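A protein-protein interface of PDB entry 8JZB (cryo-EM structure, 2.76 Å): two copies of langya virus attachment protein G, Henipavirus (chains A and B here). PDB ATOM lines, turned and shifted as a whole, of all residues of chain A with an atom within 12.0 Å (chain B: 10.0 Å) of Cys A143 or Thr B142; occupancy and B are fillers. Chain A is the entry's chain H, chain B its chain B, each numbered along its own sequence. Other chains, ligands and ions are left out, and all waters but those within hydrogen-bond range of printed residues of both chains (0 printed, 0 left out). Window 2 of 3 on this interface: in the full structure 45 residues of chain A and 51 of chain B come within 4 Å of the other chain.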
ATOM      1  N   GLU A 134     -11.154  19.562 -14.533  1.00  0.00           N
ATOM      2  CA  GLU A 134     -11.473  19.170 -13.161  1.00  0.00           C
ATOM      3  C   GLU A 134     -10.310  19.458 -12.220  1.00  0.00           C
ATOM      4  O   GLU A 134     -10.509  19.970 -11.107  1.00  0.00           O
ATOM      5  CB  GLU A 134     -11.847  17.690 -13.108  1.00  0.00           C
ATOM      6  CG  GLU A 134     -13.297  17.403 -13.450  1.00  0.00           C
ATOM      7  CD  GLU A 134     -14.160  17.237 -12.215  1.00  0.00           C
ATOM      8  OE1 GLU A 134     -13.758  17.724 -11.138  1.00  0.00           O
ATOM      9  OE2 GLU A 134     -15.239  16.619 -12.320  1.00  0.00           O
ATOM     10  N   GLU A 135      -9.087  19.135 -12.649  1.00  0.00           N
ATOM     11  CA  GLU A 135      -7.923  19.383 -11.804  1.00  0.00           C
ATOM     12  C   GLU A 135      -7.767  20.869 -11.501  1.00  0.00           C
ATOM     13  O   GLU A 135      -7.531  21.255 -10.349  1.00  0.00           O
ATOM     14  CB  GLU A 135      -6.662  18.835 -12.471  1.00  0.00           C
ATOM     15  CG  GLU A 135      -5.767  18.044 -11.536  1.00  0.00           C
ATOM     16  CD  GLU A 135      -6.439  16.793 -11.008  1.00  0.00           C
ATOM     17  OE1 GLU A 135      -6.972  16.835  -9.879  1.00  0.00           O
ATOM     18  OE2 GLU A 135      -6.430  15.766 -11.719  1.00  0.00           O
ATOM     19  N   SER A 136      -7.913  21.718 -12.521  1.00  0.00           N
ATOM     20  CA  SER A 136      -7.810  23.155 -12.304  1.00  0.00           C
ATOM     21  C   SER A 136      -8.936  23.689 -11.429  1.00  0.00           C
ATOM     22  O   SER A 136      -8.697  24.595 -10.625  1.00  0.00           O
ATOM     23  CB  SER A 136      -7.796  23.896 -13.640  1.00  0.00           C
ATOM     24  OG  SER A 136      -9.055  23.814 -14.283  1.00  0.00           O
ATOM     25  N   ILE A 137     -10.149  23.152 -11.566  1.00  0.00           N
ATOM     26  CA  ILE A 137     -11.247  23.567 -10.699  1.00  0.00           C
ATOM     27  C   ILE A 137     -10.917  23.273  -9.244  1.00  0.00           C
ATOM     28  O   ILE A 137     -11.046  24.145  -8.374  1.00  0.00           O
ATOM     29  CB  ILE A 137     -12.556  22.878 -11.127  1.00  0.00           C
ATOM     30  CG1 ILE A 137     -13.237  23.676 -12.236  1.00  0.00           C
ATOM     31  CG2 ILE A 137     -13.498  22.719  -9.940  1.00  0.00           C
ATOM     32  CD1 ILE A 137     -14.625  23.197 -12.573  1.00  0.00           C
ATOM     33  N   THR A 138     -10.458  22.051  -8.965  1.00  0.00           N
ATOM     34  CA  THR A 138     -10.119  21.685  -7.592  1.00  0.00           C
ATOM     35  C   THR A 138      -8.971  22.537  -7.066  1.00  0.00           C
ATOM     36  O   THR A 138      -8.962  22.934  -5.895  1.00  0.00           O
ATOM     37  CB  THR A 138      -9.769  20.199  -7.502  1.00  0.00           C
ATOM     38  OG1 THR A 138      -8.591  19.934  -8.273  1.00  0.00           O
ATOM     39  CG2 THR A 138     -10.920  19.343  -8.008  1.00  0.00           C
ATOM     40  N   LYS A 139      -7.987  22.830  -7.919  1.00  0.00           N
ATOM     41  CA  LYS A 139      -6.836  23.604  -7.467  1.00  0.00           C
ATOM     42  C   LYS A 139      -7.190  25.062  -7.195  1.00  0.00           C
ATOM     43  O   LYS A 139      -6.671  25.657  -6.244  1.00  0.00           O
ATOM     44  CB  LYS A 139      -5.710  23.520  -8.496  1.00  0.00           C
ATOM     45  CG  LYS A 139      -4.397  24.122  -8.025  1.00  0.00           C
ATOM     46  CD  LYS A 139      -3.303  23.942  -9.061  1.00  0.00           C
ATOM     47  CE  LYS A 139      -3.607  24.728 -10.326  1.00  0.00           C
ATOM     48  NZ  LYS A 139      -3.667  26.192 -10.065  1.00  0.00           N
ATOM     49  N   GLN A 140      -8.069  25.656  -8.005  1.00  0.00           N
ATOM     50  CA  GLN A 140      -8.313  27.092  -7.938  1.00  0.00           C
ATOM     51  C   GLN A 140      -9.534  27.492  -7.125  1.00  0.00           C
ATOM     52  O   GLN A 140      -9.417  28.370  -6.269  1.00  0.00           O
ATOM     53  CB  GLN A 140      -8.450  27.675  -9.350  1.00  0.00           C
ATOM     54  CG  GLN A 140      -7.136  28.098 -10.030  1.00  0.00           C
ATOM     55  CD  GLN A 140      -6.349  29.188  -9.294  1.00  0.00           C
ATOM     56  OE1 GLN A 140      -6.518  29.419  -8.097  1.00  0.00           O
ATOM     57  NE2 GLN A 140      -5.475  29.862 -10.030  1.00  0.00           N
ATOM     58  N   CYS A 141     -10.699  26.884  -7.356  1.00  0.00           N
ATOM     59  CA  CYS A 141     -11.912  27.284  -6.652  1.00  0.00           C
ATOM     60  C   CYS A 141     -12.038  26.614  -5.289  1.00  0.00           C
ATOM     61  O   CYS A 141     -13.144  26.539  -4.744  1.00  0.00           O
ATOM     62  CB  CYS A 141     -13.154  26.988  -7.497  1.00  0.00           C
ATOM     63  SG  CYS A 141     -13.210  27.766  -9.139  1.00  0.00           S
ATOM     64  N   THR A 142     -10.929  26.122  -4.728  1.00  0.00           N
ATOM     65  CA  THR A 142     -10.994  25.445  -3.437  1.00  0.00           C
ATOM     66  C   THR A 142     -11.361  26.411  -2.313  1.00  0.00           C
ATOM     67  O   THR A 142     -12.216  26.097  -1.476  1.00  0.00           O
ATOM     68  CB  THR A 142      -9.668  24.727  -3.150  1.00  0.00           C
ATOM     69  OG1 THR A 142      -9.747  24.043  -1.893  1.00  0.00           O
ATOM     70  CG2 THR A 142      -8.484  25.693  -3.148  1.00  0.00           C
ATOM     71  N   CYS A 143     -10.748  27.594  -2.296  1.00  0.00           N
ATOM     72  CA  CYS A 143     -10.992  28.620  -1.278  1.00  0.00           C
ATOM     73  C   CYS A 143     -11.012  28.071   0.148  1.00  0.00           C
ATOM     74  O   CYS A 143     -10.315  27.107   0.465  1.00  0.00           O
ATOM     75  CB  CYS A 143     -12.306  29.348  -1.569  1.00  0.00           C
ATOM     76  SG  CYS A 143     -13.005  30.226  -0.151  1.00  0.00           S
ATOM     77  N   SER B 136     -11.707  31.935 -17.821  1.00  0.00           N
ATOM     78  CA  SER B 136     -12.786  32.435 -16.975  1.00  0.00           C
ATOM     79  C   SER B 136     -12.712  31.847 -15.571  1.00  0.00           C
ATOM     80  O   SER B 136     -12.959  32.548 -14.584  1.00  0.00           O
ATOM     81  CB  SER B 136     -14.136  32.121 -17.614  1.00  0.00           C
ATOM     82  OG  SER B 136     -15.118  31.871 -16.627  1.00  0.00           O
ATOM     83  N   ILE B 137     -12.381  30.559 -15.465  1.00  0.00           N
ATOM     84  CA  ILE B 137     -12.289  29.913 -14.159  1.00  0.00           C
ATOM     85  C   ILE B 137     -11.182  30.553 -13.333  1.00  0.00           C
ATOM     86  O   ILE B 137     -11.356  30.839 -12.143  1.00  0.00           O
ATOM     87  CB  ILE B 137     -12.065  28.401 -14.332  1.00  0.00           C
ATOM     88  CG1 ILE B 137     -13.403  27.690 -14.521  1.00  0.00           C
ATOM     89  CG2 ILE B 137     -11.332  27.824 -13.133  1.00  0.00           C
ATOM     90  CD1 ILE B 137     -13.282  26.196 -14.647  1.00  0.00           C
ATOM     91  N   THR B 138     -10.024  30.786 -13.954  1.00  0.00           N
ATOM     92  CA  THR B 138      -8.920  31.412 -13.231  1.00  0.00           C
ATOM     93  C   THR B 138      -9.270  32.834 -12.808  1.00  0.00           C
ATOM     94  O   THR B 138      -8.915  33.269 -11.707  1.00  0.00           O
ATOM     95  CB  THR B 138      -7.651  31.403 -14.083  1.00  0.00           C
ATOM     96  OG1 THR B 138      -7.884  32.128 -15.298  1.00  0.00           O
ATOM     97  CG2 THR B 138      -7.233  29.976 -14.406  1.00  0.00           C
ATOM     98  N   LYS B 139      -9.966  33.576 -13.672  1.00  0.00           N
ATOM     99  CA  LYS B 139     -10.235  34.981 -13.376  1.00  0.00           C
ATOM    100  C   LYS B 139     -11.306  35.135 -12.300  1.00  0.00           C
ATOM    101  O   LYS B 139     -11.187  35.983 -11.408  1.00  0.00           O
ATOM    102  CB  LYS B 139     -10.643  35.716 -14.655  1.00  0.00           C
ATOM    103  CG  LYS B 139     -11.763  36.727 -14.467  1.00  0.00           C
ATOM    104  CD  LYS B 139     -11.944  37.595 -15.698  1.00  0.00           C
ATOM    105  CE  LYS B 139     -12.926  38.724 -15.433  1.00  0.00           C
ATOM    106  NZ  LYS B 139     -12.358  39.758 -14.527  1.00  0.00           N
ATOM    107  N   GLN B 140     -12.360  34.317 -12.359  1.00  0.00           N
ATOM    108  CA  GLN B 140     -13.529  34.568 -11.520  1.00  0.00           C
ATOM    109  C   GLN B 140     -13.340  34.019 -10.110  1.00  0.00           C
ATOM    110  O   GLN B 140     -13.621  34.711  -9.125  1.00  0.00           O
ATOM    111  CB  GLN B 140     -14.775  33.969 -12.173  1.00  0.00           C
ATOM    112  CG  GLN B 140     -15.876  34.982 -12.440  1.00  0.00           C
ATOM    113  CD  GLN B 140     -16.621  35.374 -11.181  1.00  0.00           C
ATOM    114  OE1 GLN B 140     -16.716  34.592 -10.236  1.00  0.00           O
ATOM    115  NE2 GLN B 140     -17.154  36.590 -11.161  1.00  0.00           N
ATOM    116  N   CYS B 141     -12.869  32.781  -9.991  1.00  0.00           N
ATOM    117  CA  CYS B 141     -12.735  32.156  -8.683  1.00  0.00           C
ATOM    118  C   CYS B 141     -11.608  32.801  -7.880  1.00  0.00           C
ATOM    119  O   CYS B 141     -10.671  33.392  -8.426  1.00  0.00           O
ATOM    120  CB  CYS B 141     -12.481  30.657  -8.825  1.00  0.00           C
ATOM    121  SG  CYS B 141     -13.970  29.629  -8.832  1.00  0.00           S
ATOM    122  N   THR B 142     -11.711  32.676  -6.558  1.00  0.00           N
ATOM    123  CA  THR B 142     -10.751  33.260  -5.635  1.00  0.00           C
ATOM    124  C   THR B 142     -10.304  32.212  -4.626  1.00  0.00           C
ATOM    125  O   THR B 142     -11.060  31.310  -4.257  1.00  0.00           O
ATOM    126  CB  THR B 142     -11.354  34.479  -4.914  1.00  0.00           C
ATOM    127  OG1 THR B 142     -12.534  34.084  -4.206  1.00  0.00           O
ATOM    128  CG2 THR B 142     -11.872  35.494  -5.921  1.00  0.00           C
ATOM    129  N   CYS B 143      -9.055  32.350  -4.185  1.00  0.00           N
ATOM    130  CA  CYS B 143      -8.453  31.466  -3.189  1.00  0.00           C
ATOM    131  C   CYS B 143      -8.559  29.997  -3.590  1.00  0.00           C
ATOM    132  O   CYS B 143      -8.088  29.111  -2.875  1.00  0.00           O
ATOM    133  CB  CYS B 143      -9.107  31.681  -1.823  1.00  0.00           C
ATOM    134  SG  CYS B 143      -8.838  33.323  -1.117  1.00  0.00           S
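O of Cys B143 is in hydrogen-bond range of N of Cys A143 (3.1 Å).
The side-chain sulfur (SG) of Cys B141 is disulfide-bonded to the side-chain sulfur (SG) of Cys A141, 2.0 Å away.
Among the printed residues, merely in contact across the chains: Gln A140 with Cys B143 (3.2 Å), Thr A142 with Cys B143 (3.5 Å), Ile A137 with Ile B137 (3.5 Å), Cys A143 with Thr B142 (3.6 Å) and Gln A140 with Thr B142 (3.9 Å).
Thr B142 touches just these residues of chain A: Gln A140 (3.9 Å) and Cys A143 (3.6 Å).
Cys A141 touches just one residue of chain B: Cys B141.
Thr A142 touches one residue of chain B.
No residue of chain A comes within 4 Å of Gln B140.
Of chain A, only Cys A141 comes within 4 Å of Cys B141.
Of the printed residues of chain A, Cys B143 touches Gln A140 (3.2 Å), Thr A142 (3.5 Å) and Cys A143 (3.1 Å).
Of the printed residues of chain B, Gln A140 touches Thr B142 (3.9 Å) and Cys B143 (3.2 Å).
Of the printed residues of chain B, Ile A137 touches Ile B137.
Printed residues of chain A within 4 Å of Ile B137: Ile A137.
Ser B136 touches none of the printed residues of chain A.
Thr B138 touches none of the printed residues of chain A.
The nearest residue of chain B that does not touch Cys A143 is Cys B141 (7.2 Å).
The nearest residue of chain A that does not touch Thr B142 is Cys A141 (4.8 Å).
The nearest printed residue of chain B that does not touch Ile A137 is Cys B141 (6.2 Å).
Hydrophobic or aromatic side chains of chain B that line the printed part of chain A: Ile B137.
Among the printed residues, 7 pairs touch across the chains.
Among the printed residues, no Asp or Glu carboxylate lies within 4 Å of a Lys or Arg side-chain nitrogen of the other chain.
Ile A137 touches its own counterpart, Ile B137.
Gln A140 touches Cys B143, but with the chains exchanged Cys A143 does not touch Gln B140 (9.4 Å).
Cys B141 touches its own counterpart, Cys A141.
Thr A142 touches Cys B143, and with the chains exchanged Cys A143 touches Thr B142.
Of the 7 pairs that touch across the chains among the printed residues, 5 have their exchanged pair printed and touching as well.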
